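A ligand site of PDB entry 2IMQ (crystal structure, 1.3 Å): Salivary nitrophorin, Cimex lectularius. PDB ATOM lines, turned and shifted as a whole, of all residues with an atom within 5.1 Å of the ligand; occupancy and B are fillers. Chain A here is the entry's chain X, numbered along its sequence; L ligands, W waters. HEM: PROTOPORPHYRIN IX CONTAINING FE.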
ATOM      1  N   TRP A  14     -31.102   9.698  19.740  1.00  0.00           N
ATOM      2  CA  TRP A  14     -29.908   8.904  19.536  1.00  0.00           C
ATOM      3  C   TRP A  14     -29.379   8.468  20.871  1.00  0.00           C
ATOM      4  O   TRP A  14     -29.059   9.281  21.731  1.00  0.00           O
ATOM      5  CB  TRP A  14     -28.891   9.764  18.832  1.00  0.00           C
ATOM      6  CG  TRP A  14     -27.726   9.063  18.272  1.00  0.00           C
ATOM      7  CD1 TRP A  14     -27.460   7.725  18.220  1.00  0.00           C
ATOM      8  CD2 TRP A  14     -26.707   9.706  17.525  1.00  0.00           C
ATOM      9  NE1 TRP A  14     -26.276   7.518  17.550  1.00  0.00           N
ATOM     10  CE2 TRP A  14     -25.808   8.730  17.114  1.00  0.00           C
ATOM     11  CE3 TRP A  14     -26.467  11.034  17.176  1.00  0.00           C
ATOM     12  CZ2 TRP A  14     -24.686   9.044  16.355  1.00  0.00           C
ATOM     13  CZ3 TRP A  14     -25.362  11.329  16.452  1.00  0.00           C
ATOM     14  CH2 TRP A  14     -24.505  10.350  16.036  1.00  0.00           C
ATOM     15  N   SER A  16     -26.440   7.833  22.046  1.00  0.00           N
ATOM     16  CA  SER A  16     -25.121   8.223  21.545  1.00  0.00           C
ATOM     17  C   SER A  16     -23.995   7.851  22.510  1.00  0.00           C
ATOM     18  O   SER A  16     -22.807   7.865  22.129  1.00  0.00           O
ATOM     19  CB  SER A  16     -25.157   9.740  21.283  1.00  0.00           C
ATOM     20  OG  SER A  16     -25.602  10.394  22.435  1.00  0.00           O
ATOM     21  N   GLY A  17     -24.288   7.464  23.749  1.00  0.00           N
ATOM     22  CA  GLY A  17     -23.235   6.963  24.630  1.00  0.00           C
ATOM     23  C   GLY A  17     -22.277   8.059  25.031  1.00  0.00           C
ATOM     24  O   GLY A  17     -22.705   9.109  25.508  1.00  0.00           O
ATOM     25  N   HIS A  18     -20.977   7.806  24.798  1.00  0.00           N
ATOM     26  CA  HIS A  18     -19.945   8.796  25.076  1.00  0.00           C
ATOM     27  C   HIS A  18     -19.605   9.619  23.836  1.00  0.00           C
ATOM     28  O   HIS A  18     -18.689  10.449  23.884  1.00  0.00           O
ATOM     29  CB  HIS A  18     -18.674   8.115  25.645  1.00  0.00           C
ATOM     30  CG  HIS A  18     -18.875   7.500  26.995  1.00  0.00           C
ATOM     31  ND1 HIS A  18     -18.361   8.044  28.156  1.00  0.00           N
ATOM     32  CD2 HIS A  18     -19.545   6.382  27.380  1.00  0.00           C
ATOM     33  CE1 HIS A  18     -18.689   7.290  29.183  1.00  0.00           C
ATOM     34  NE2 HIS A  18     -19.413   6.275  28.747  1.00  0.00           N
ATOM     35  N   GLU A  19     -20.332   9.461  22.736  1.00  0.00           N
ATOM     36  CA  GLU A  19     -19.975  10.175  21.503  1.00  0.00           C
ATOM     37  C   GLU A  19     -20.357  11.644  21.536  1.00  0.00           C
ATOM     38  O   GLU A  19     -21.445  11.998  21.948  1.00  0.00           O
ATOM     39  CB  GLU A  19     -20.519   9.529  20.244  1.00  0.00           C
ATOM     40  CG  GLU A  19     -19.403   9.158  19.257  1.00  0.00           C
ATOM     41  CD  GLU A  19     -19.596   9.834  17.923  1.00  0.00           C
ATOM     42  OE1 GLU A  19     -18.585  10.145  17.254  1.00  0.00           O
ATOM     43  OE2 GLU A  19     -20.770  10.098  17.563  1.00  0.00           O
ATOM     44  N   ARG A  20     -19.442  12.497  21.086  1.00  0.00           N
ATOM     45  CA  ARG A  20     -19.731  13.898  20.868  1.00  0.00           C
ATOM     46  C   ARG A  20     -20.759  14.142  19.780  1.00  0.00           C
ATOM     47  O   ARG A  20     -20.915  13.333  18.868  1.00  0.00           O
ATOM     48  CB  ARG A  20     -18.465  14.651  20.493  1.00  0.00           C
ATOM     49  CG  ARG A  20     -17.875  14.306  19.152  1.00  0.00           C
ATOM     50  CD  ARG A  20     -16.634  15.082  18.851  1.00  0.00           C
ATOM     51  NE  ARG A  20     -15.986  14.678  17.613  1.00  0.00           N
ATOM     52  CZ  ARG A  20     -14.819  15.165  17.174  1.00  0.00           C
ATOM     53  NH1 ARG A  20     -14.155  16.086  17.889  1.00  0.00           N
ATOM     54  NH2 ARG A  20     -14.287  14.736  16.034  1.00  0.00           N
ATOM     55  N   ALA A  21     -21.480  15.246  19.864  1.00  0.00           N
ATOM     56  CA  ALA A  21     -22.363  15.619  18.786  1.00  0.00           C
ATOM     57  C   ALA A  21     -21.601  15.714  17.481  1.00  0.00           C
ATOM     58  O   ALA A  21     -20.455  16.233  17.445  1.00  0.00           O
ATOM     59  CB  ALA A  21     -23.060  16.918  19.064  1.00  0.00           C
ATOM     60  N   PRO A  22     -22.217  15.251  16.395  1.00  0.00           N
ATOM     61  CA  PRO A  22     -21.633  15.427  15.090  1.00  0.00           C
ATOM     62  C   PRO A  22     -21.679  16.887  14.707  1.00  0.00           C
ATOM     63  O   PRO A  22     -22.380  17.682  15.325  1.00  0.00           O
ATOM     64  CB  PRO A  22     -22.499  14.556  14.178  1.00  0.00           C
ATOM     65  CG  PRO A  22     -23.748  14.425  14.857  1.00  0.00           C
ATOM     66  CD  PRO A  22     -23.512  14.545  16.323  1.00  0.00           C
ATOM     67  N   LEU A  28     -29.178  15.234  10.417  1.00  0.00           N
ATOM     68  CA  LEU A  28     -29.664  14.715  11.692  1.00  0.00           C
ATOM     69  C   LEU A  28     -31.051  15.244  12.021  1.00  0.00           C
ATOM     70  O   LEU A  28     -31.877  14.536  12.574  1.00  0.00           O
ATOM     71  CB  LEU A  28     -28.656  15.096  12.790  1.00  0.00           C
ATOM     72  CG  LEU A  28     -28.946  14.464  14.123  1.00  0.00           C
ATOM     73  CD1 LEU A  28     -28.671  12.995  14.148  1.00  0.00           C
ATOM     74  CD2 LEU A  28     -28.209  15.138  15.241  1.00  0.00           C
ATOM     75  N   VAL A  42     -34.704  17.276  19.990  1.00  0.00           N
ATOM     76  CA  VAL A  42     -33.513  16.428  19.974  1.00  0.00           C
ATOM     77  C   VAL A  42     -33.307  15.755  21.319  1.00  0.00           C
ATOM     78  O   VAL A  42     -33.166  16.445  22.323  1.00  0.00           O
ATOM     79  CB  VAL A  42     -32.249  17.290  19.658  1.00  0.00           C
ATOM     80  CG1 VAL A  42     -31.011  16.399  19.579  1.00  0.00           C
ATOM     81  CG2 VAL A  42     -32.483  18.090  18.340  1.00  0.00           C
ATOM     82  N   VAL A  44     -31.038  12.811  23.441  1.00  0.00           N
ATOM     83  CA  VAL A  44     -29.886  11.915  23.489  1.00  0.00           C
ATOM     84  C   VAL A  44     -29.842  11.165  24.805  1.00  0.00           C
ATOM     85  O   VAL A  44     -30.346  11.627  25.821  1.00  0.00           O
ATOM     86  CB  VAL A  44     -28.557  12.615  23.280  1.00  0.00           C
ATOM     87  CG1 VAL A  44     -28.426  13.060  21.924  1.00  0.00           C
ATOM     88  CG2 VAL A  44     -28.361  13.752  24.226  1.00  0.00           C
ATOM     89  N   PHE A  47     -23.704   9.185  28.489  1.00  0.00           N
ATOM     90  CA  PHE A  47     -22.967   9.219  29.770  1.00  0.00           C
ATOM     91  C   PHE A  47     -22.174  10.486  29.929  1.00  0.00           C
ATOM     92  O   PHE A  47     -21.493  10.909  29.003  1.00  0.00           O
ATOM     93  CB  PHE A  47     -22.008   8.052  29.838  1.00  0.00           C
ATOM     94  CG  PHE A  47     -22.698   6.729  29.938  1.00  0.00           C
ATOM     95  CD1 PHE A  47     -22.821   5.928  28.804  1.00  0.00           C
ATOM     96  CD2 PHE A  47     -23.290   6.319  31.129  1.00  0.00           C
ATOM     97  CE1 PHE A  47     -23.510   4.709  28.879  1.00  0.00           C
ATOM     98  CE2 PHE A  47     -23.966   5.104  31.214  1.00  0.00           C
ATOM     99  CZ  PHE A  47     -24.075   4.291  30.087  1.00  0.00           C
ATOM    100  N   GLY A  48     -22.252  11.045  31.125  1.00  0.00           N
ATOM    101  CA  GLY A  48     -21.375  12.160  31.529  1.00  0.00           C
ATOM    102  C   GLY A  48     -21.764  13.518  30.981  1.00  0.00           C
ATOM    103  O   GLY A  48     -20.946  14.443  30.992  1.00  0.00           O
ATOM    104  N   PHE A  49     -22.992  13.703  30.532  1.00  0.00           N
ATOM    105  CA  PHE A  49     -23.370  14.988  29.946  1.00  0.00           C
ATOM    106  C   PHE A  49     -23.202  16.189  30.887  1.00  0.00           C
ATOM    107  O   PHE A  49     -22.666  17.189  30.458  1.00  0.00           O
ATOM    108  CB  PHE A  49     -24.823  14.994  29.482  1.00  0.00           C
ATOM    109  CG  PHE A  49     -25.114  13.987  28.404  1.00  0.00           C
ATOM    110  CD1 PHE A  49     -26.241  13.198  28.481  1.00  0.00           C
ATOM    111  CD2 PHE A  49     -24.301  13.871  27.307  1.00  0.00           C
ATOM    112  CE1 PHE A  49     -26.523  12.285  27.501  1.00  0.00           C
ATOM    113  CE2 PHE A  49     -24.619  12.965  26.265  1.00  0.00           C
ATOM    114  CZ  PHE A  49     -25.731  12.174  26.398  1.00  0.00           C
ATOM    115  N   GLN A  50     -23.716  16.070  32.109  1.00  0.00           N
ATOM    116  CA  GLN A  50     -23.770  17.164  33.074  1.00  0.00           C
ATOM    117  C   GLN A  50     -22.369  17.486  33.558  1.00  0.00           C
ATOM    118  O   GLN A  50     -21.924  18.639  33.480  1.00  0.00           O
ATOM    119  CB  GLN A  50     -24.681  16.753  34.239  1.00  0.00           C
ATOM    120  CG  GLN A  50     -25.051  17.839  35.224  1.00  0.00           C
ATOM    121  CD  GLN A  50     -26.334  17.507  35.977  1.00  0.00           C
ATOM    122  OE1 GLN A  50     -27.025  18.401  36.446  1.00  0.00           O
ATOM    123  NE2 GLN A  50     -26.647  16.211  36.080  1.00  0.00           N
ATOM    124  N   ASP A  52     -19.684  16.733  32.102  1.00  0.00           N
ATOM    125  CA  ASP A  52     -19.053  17.180  30.861  1.00  0.00           C
ATOM    126  C   ASP A  52     -17.524  17.234  30.943  1.00  0.00           C
ATOM    127  O   ASP A  52     -16.907  18.224  30.562  1.00  0.00           O
ATOM    128  CB  ASP A  52     -19.628  18.518  30.388  1.00  0.00           C
ATOM    129  CG  ASP A  52     -19.184  18.883  28.976  1.00  0.00           C
ATOM    130  OD1 ASP A  52     -19.382  20.032  28.537  1.00  0.00           O
ATOM    131  OD2 ASP A  52     -18.608  18.065  28.220  1.00  0.00           O
ATOM    132  N   PRO A  54     -15.399  15.716  28.926  1.00  0.00           N
ATOM    133  CA  PRO A  54     -14.862  15.972  27.598  1.00  0.00           C
ATOM    134  C   PRO A  54     -14.916  17.452  27.143  1.00  0.00           C
ATOM    135  O   PRO A  54     -14.277  17.805  26.149  1.00  0.00           O
ATOM    136  CB  PRO A  54     -15.757  15.102  26.693  1.00  0.00           C
ATOM    137  CG  PRO A  54     -16.372  14.129  27.580  1.00  0.00           C
ATOM    138  CD  PRO A  54     -16.566  14.817  28.886  1.00  0.00           C
ATOM    139  N   GLN A  56     -17.547  19.072  25.788  1.00  0.00           N
ATOM    140  CA  GLN A  56     -18.147  19.080  24.459  1.00  0.00           C
ATOM    141  C   GLN A  56     -19.450  19.956  24.438  1.00  0.00           C
ATOM    142  O   GLN A  56     -19.968  20.335  23.412  1.00  0.00           O
ATOM    143  CB  GLN A  56     -18.356  17.626  23.981  1.00  0.00           C
ATOM    144  CG  GLN A  56     -18.328  17.489  22.475  1.00  0.00           C
ATOM    145  CD  GLN A  56     -19.683  17.752  21.833  1.00  0.00           C
ATOM    146  OE1 GLN A  56     -19.757  18.254  20.714  1.00  0.00           O
ATOM    147  NE2 GLN A  56     -20.762  17.432  22.548  1.00  0.00           N
ATOM    148  N   GLY A  57     -19.965  20.225  25.614  1.00  0.00           N
ATOM    149  CA  GLY A  57     -21.067  21.171  25.769  1.00  0.00           C
ATOM    150  C   GLY A  57     -20.884  22.427  24.935  1.00  0.00           C
ATOM    151  O   GLY A  57     -21.796  22.793  24.164  1.00  0.00           O
ATOM    152  N   PRO A  58     -19.774  23.170  25.095  1.00  0.00           N
ATOM    153  CA  PRO A  58     -19.560  24.361  24.287  1.00  0.00           C
ATOM    154  C   PRO A  58     -19.756  24.182  22.773  1.00  0.00           C
ATOM    155  O   PRO A  58     -20.368  25.058  22.162  1.00  0.00           O
ATOM    156  CB  PRO A  58     -18.123  24.773  24.639  1.00  0.00           C
ATOM    157  CG  PRO A  58     -17.956  24.335  26.017  1.00  0.00           C
ATOM    158  CD  PRO A  58     -18.730  22.995  26.120  1.00  0.00           C
ATOM    159  N   CYS A  60     -21.534  21.876  21.208  1.00  0.00           N
ATOM    160  CA  CYS A  60     -22.931  21.573  20.974  1.00  0.00           C
ATOM    161  C   CYS A  60     -23.681  22.893  20.843  1.00  0.00           C
ATOM    162  O   CYS A  60     -24.407  23.119  19.880  1.00  0.00           O
ATOM    163  CB  CYS A  60     -23.511  20.759  22.122  1.00  0.00           C
ATOM    164  SG  CYS A  60     -22.979  19.103  22.111  1.00  0.00           S
ATOM    165  N   VAL A  61     -23.487  23.775  21.810  1.00  0.00           N
ATOM    166  CA  VAL A  61     -24.227  25.031  21.819  1.00  0.00           C
ATOM    167  C   VAL A  61     -23.857  25.831  20.592  1.00  0.00           C
ATOM    168  O   VAL A  61     -24.690  26.297  19.862  1.00  0.00           O
ATOM    169  CB  VAL A  61     -23.938  25.836  23.115  1.00  0.00           C
ATOM    170  CG1 VAL A  61     -24.626  27.191  23.098  1.00  0.00           C
ATOM    171  CG2 VAL A  61     -24.385  25.120  24.335  1.00  0.00           C
ATOM    172  N   PHE A  64     -25.222  23.920  17.143  1.00  0.00           N
ATOM    173  CA  PHE A  64     -26.666  23.904  17.029  1.00  0.00           C
ATOM    174  C   PHE A  64     -27.208  25.319  16.886  1.00  0.00           C
ATOM    175  O   PHE A  64     -28.046  25.578  15.991  1.00  0.00           O
ATOM    176  CB  PHE A  64     -27.355  23.177  18.185  1.00  0.00           C
ATOM    177  CG  PHE A  64     -27.410  21.694  17.995  1.00  0.00           C
ATOM    178  CD1 PHE A  64     -26.394  20.894  18.513  1.00  0.00           C
ATOM    179  CD2 PHE A  64     -28.438  21.119  17.269  1.00  0.00           C
ATOM    180  CE1 PHE A  64     -26.469  19.517  18.349  1.00  0.00           C
ATOM    181  CE2 PHE A  64     -28.514  19.735  17.064  1.00  0.00           C
ATOM    182  CZ  PHE A  64     -27.517  18.957  17.604  1.00  0.00           C
ATOM    183  N   GLN A  65     -26.693  26.233  17.709  1.00  0.00           N
ATOM    184  CA  GLN A  65     -27.233  27.615  17.684  1.00  0.00           C
ATOM    185  C   GLN A  65     -26.836  28.303  16.370  1.00  0.00           C
ATOM    186  O   GLN A  65     -27.663  28.953  15.761  1.00  0.00           O
ATOM    187  CB  GLN A  65     -26.831  28.419  18.943  1.00  0.00           C
ATOM    188  CG  GLN A  65     -27.066  27.768  20.301  1.00  0.00           C
ATOM    189  CD  GLN A  65     -28.425  27.953  20.953  1.00  0.00           C
ATOM    190  OE1 GLN A  65     -29.474  27.697  20.350  1.00  0.00           O
ATOM    191  NE2 GLN A  65     -28.382  28.287  22.264  1.00  0.00           N
ATOM    192  N   LYS A  75     -34.510  28.372  20.725  1.00  0.00           N
ATOM    193  CA  LYS A  75     -34.361  27.212  21.640  1.00  0.00           C
ATOM    194  C   LYS A  75     -35.278  27.473  22.844  1.00  0.00           C
ATOM    195  O   LYS A  75     -35.046  28.429  23.611  1.00  0.00           O
ATOM    196  CB  LYS A  75     -32.920  27.039  22.095  1.00  0.00           C
ATOM    197  CG  LYS A  75     -32.795  25.946  23.165  1.00  0.00           C
ATOM    198  CD  LYS A  75     -31.394  25.796  23.627  1.00  0.00           C
ATOM    199  CE  LYS A  75     -30.972  26.898  24.554  1.00  0.00           C
ATOM    200  NZ  LYS A  75     -29.554  26.747  24.880  1.00  0.00           N
ATOM    201  N   ASN A  78     -33.081  23.558  26.701  1.00  0.00           N
ATOM    202  CA  ASN A  78     -32.189  22.388  26.792  1.00  0.00           C
ATOM    203  C   ASN A  78     -32.133  21.937  28.211  1.00  0.00           C
ATOM    204  O   ASN A  78     -31.981  22.778  29.133  1.00  0.00           O
ATOM    205  CB  ASN A  78     -30.768  22.720  26.327  1.00  0.00           C
ATOM    206  CG  ASN A  78     -29.755  21.650  26.647  1.00  0.00           C
ATOM    207  OD1 ASN A  78     -29.002  21.757  27.619  1.00  0.00           O
ATOM    208  ND2 ASN A  78     -29.790  20.567  25.878  1.00  0.00           N
ATOM    209  N   ILE A  80     -30.202  18.834  30.528  1.00  0.00           N
ATOM    210  CA  ILE A  80     -29.327  17.682  30.632  1.00  0.00           C
ATOM    211  C   ILE A  80     -29.246  17.123  32.037  1.00  0.00           C
ATOM    212  O   ILE A  80     -29.283  17.857  33.063  1.00  0.00           O
ATOM    213  CB  ILE A  80     -27.912  17.958  30.067  1.00  0.00           C
ATOM    214  CG1 ILE A  80     -27.210  19.042  30.882  1.00  0.00           C
ATOM    215  CG2 ILE A  80     -27.984  18.288  28.580  1.00  0.00           C
ATOM    216  CD1 ILE A  80     -25.758  19.320  30.429  1.00  0.00           C
ATOM    217  N   THR A  87     -33.643  18.772  24.013  1.00  0.00           N
ATOM    218  CA  THR A  87     -33.693  20.153  23.550  1.00  0.00           C
ATOM    219  C   THR A  87     -34.914  20.284  22.662  1.00  0.00           C
ATOM    220  O   THR A  87     -35.145  19.456  21.789  1.00  0.00           O
ATOM    221  CB  THR A  87     -32.418  20.503  22.790  1.00  0.00           C
ATOM    222  OG1 THR A  87     -31.271  20.188  23.589  1.00  0.00           O
ATOM    223  CG2 THR A  87     -32.376  21.995  22.484  1.00  0.00           C
ATOM    224  N   TYR A  89     -36.726  23.175  20.040  1.00  0.00           N
ATOM    225  CA  TYR A  89     -36.658  24.413  19.280  1.00  0.00           C
ATOM    226  C   TYR A  89     -37.995  24.657  18.625  1.00  0.00           C
ATOM    227  O   TYR A  89     -38.701  23.727  18.216  1.00  0.00           O
ATOM    228  CB  TYR A  89     -35.599  24.289  18.169  1.00  0.00           C
ATOM    229  CG  TYR A  89     -34.233  24.001  18.608  1.00  0.00           C
ATOM    230  CD1 TYR A  89     -33.774  22.710  18.644  1.00  0.00           C
ATOM    231  CD2 TYR A  89     -33.356  25.000  18.977  1.00  0.00           C
ATOM    232  CE1 TYR A  89     -32.480  22.423  19.030  1.00  0.00           C
ATOM    233  CE2 TYR A  89     -32.055  24.721  19.361  1.00  0.00           C
ATOM    234  CZ  TYR A  89     -31.614  23.401  19.383  1.00  0.00           C
ATOM    235  OH  TYR A  89     -30.345  23.105  19.810  1.00  0.00           O
HETATM  236  CHA HEM L   1     -26.142  20.917  24.822  1.00  0.00           C
HETATM  237  CHB HEM L   1     -27.001  17.599  21.391  1.00  0.00           C
HETATM  238  CHC HEM L   1     -23.389  14.905  23.106  1.00  0.00           C
HETATM  239  CHD HEM L   1     -22.705  17.963  26.694  1.00  0.00           C
HETATM  240  C1A HEM L   1     -26.680  20.301  23.735  1.00  0.00           C
HETATM  241  C2A HEM L   1     -27.738  20.798  22.887  1.00  0.00           C
HETATM  242  C3A HEM L   1     -27.979  19.845  21.957  1.00  0.00           C
HETATM  243  C4A HEM L   1     -27.074  18.756  22.173  1.00  0.00           C
HETATM  244  CMA HEM L   1     -28.989  19.940  20.826  1.00  0.00           C
HETATM  245  CAA HEM L   1     -28.462  22.156  22.991  1.00  0.00           C
HETATM  246  CBA HEM L   1     -27.692  23.059  21.991  1.00  0.00           C
HETATM  247  CGA HEM L   1     -28.213  24.489  22.016  1.00  0.00           C
HETATM  248  O1A HEM L   1     -27.843  25.236  22.917  1.00  0.00           O
HETATM  249  O2A HEM L   1     -28.938  24.909  21.073  1.00  0.00           O
HETATM  250  C1B HEM L   1     -26.090  16.604  21.554  1.00  0.00           C
HETATM  251  C2B HEM L   1     -25.966  15.442  20.707  1.00  0.00           C
HETATM  252  C3B HEM L   1     -24.963  14.697  21.172  1.00  0.00           C
HETATM  253  C4B HEM L   1     -24.421  15.364  22.317  1.00  0.00           C
HETATM  254  CMB HEM L   1     -26.905  15.318  19.564  1.00  0.00           C
HETATM  255  CAB HEM L   1     -24.447  13.364  20.644  1.00  0.00           C
HETATM  256  CBB HEM L   1     -24.684  12.972  19.387  1.00  0.00           C
HETATM  257  C1C HEM L   1     -22.828  15.477  24.212  1.00  0.00           C
HETATM  258  C2C HEM L   1     -21.786  14.935  25.040  1.00  0.00           C
HETATM  259  C3C HEM L   1     -21.564  15.829  25.997  1.00  0.00           C
HETATM  260  C4C HEM L   1     -22.528  16.869  25.886  1.00  0.00           C
HETATM  261  CMC HEM L   1     -20.942  13.679  24.759  1.00  0.00           C
HETATM  262  CAC HEM L   1     -20.522  15.727  27.104  1.00  0.00           C
HETATM  263  CBC HEM L   1     -20.510  14.726  27.977  1.00  0.00           C
HETATM  264  C1D HEM L   1     -23.600  19.000  26.541  1.00  0.00           C
HETATM  265  C2D HEM L   1     -23.771  20.074  27.486  1.00  0.00           C
HETATM  266  C3D HEM L   1     -24.789  20.988  26.908  1.00  0.00           C
HETATM  267  C4D HEM L   1     -25.196  20.397  25.661  1.00  0.00           C
HETATM  268  CMD HEM L   1     -23.015  20.263  28.803  1.00  0.00           C
HETATM  269  CAD HEM L   1     -25.283  22.265  27.596  1.00  0.00           C
HETATM  270  CBD HEM L   1     -24.121  23.248  27.555  1.00  0.00           C
HETATM  271  CGD HEM L   1     -24.581  24.628  27.883  1.00  0.00           C
HETATM  272  O1D HEM L   1     -23.696  25.546  27.886  1.00  0.00           O
HETATM  273  O2D HEM L   1     -25.804  24.786  28.138  1.00  0.00           O
HETATM  274  NA  HEM L   1     -26.265  19.045  23.272  1.00  0.00           N
HETATM  275  NB  HEM L   1     -25.150  16.517  22.544  1.00  0.00           N
HETATM  276  NC  HEM L   1     -23.268  16.640  24.776  1.00  0.00           N
HETATM  277  ND  HEM L   1     -24.486  19.216  25.484  1.00  0.00           N
HETATM  278 FE   HEM L   1     -24.690  17.928  23.948  1.00  0.00          FE
HETATM  279  O   HOH W   1     -28.551  17.672  24.983  1.00  0.00           O
HETATM  280  O   HOH W   2     -27.851  24.558  25.512  1.00  0.00           O
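OH of Tyr 89 lies within hydrogen-bond range of O2A of the ligand (2.6 Å).
The side-chain sulfur (SG) of Cys 60 binds an iron atom (FE) of the ligand (2.8 Å).
O2A of the ligand sits close to OE1 of Gln 65, 2.9 Å away.
The side-chain amino group of Lys 75 lies within salt-bridge range of an oxygen (O1A) of the ligand (3.0 Å).
SG of Cys 60 sits close to NE2 of Gln 56, 2.8 Å away.
The side-chain amino group of Lys 75 lies close to the side-chain amide nitrogen of Gln 65 (3.3 Å).
OD2 of Asp 52 lies within hydrogen-bond range of N of Gln 56 (2.8 Å).
N of Gly 57 lies within hydrogen-bond range of OD1 of Asp 52, 3.0 Å away.
The side-chain amide nitrogen (ND2) of Asn 78 sits at hydrogen-bond distance from the side-chain hydroxyl (OG1) of Thr 87 (2.8 Å).
The backbone carbonyl oxygen of Thr 87 sits at hydrogen-bond distance from the backbone NH of Val 42, 2.9 Å away.
NE2 of Gln 56 sits close to NC of the ligand (3.4 Å).
CZ3 of Trp 14 touches CBB of the ligand, at 3.4 Å.
Ser 16 touches the ligand (OG to CAB, 3.7 Å).
Glu 19 touches the ligand (O to CMC, 3.3 Å).
O of Arg 20 touches CBB of the ligand (3.8 Å).
CA of Ala 21 touches CBB of the ligand, at 3.6 Å.
CD of Pro 22 touches CBB of the ligand, at 3.6 Å.
Val 44 touches the ligand.
Gly 48 touches the ligand.
Phe 49 touches the ligand.
Asp 52 touches the ligand (OD2 to CAC, 3.2 Å).
Gly 57 touches the ligand (CA to C2D, 3.4 Å).
Val 61 touches the ligand (CG2 to CGD, 3.6 Å).
Phe 64 touches the ligand.
ND2 of Asn 78 touches CAA of the ligand, at 3.6 Å.
CD1 of Ile 80 touches CMD of the ligand, at 3.3 Å.
Thr 87 touches the ligand (OG1 to CAA, 3.5 Å).
Hydrophobic or aromatic side chains within 4 Å of the ligand: Trp 14, Ala 21, Pro 22, Val 44, Phe 49, Val 61, Phe 64, Ile 80 and Tyr 89.
Within 4 Å of the ligand: Trp 14, Ser 16, Glu 19, Arg 20, Ala 21, Pro 22, Val 44, Gly 48, Phe 49, Asp 52, Gln 56, Gly 57, Cys 60, Val 61, Phe 64, Gln 65, Lys 75, Asn 78, Ile 80, Thr 87 and Tyr 89.
The nearest printed residue that does not touch the ligand is His 18 (4.03 Å).
Water W2 bridges O1A of the ligand (2.7 Å) and NZ of Lys 75 (2.8 Å).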
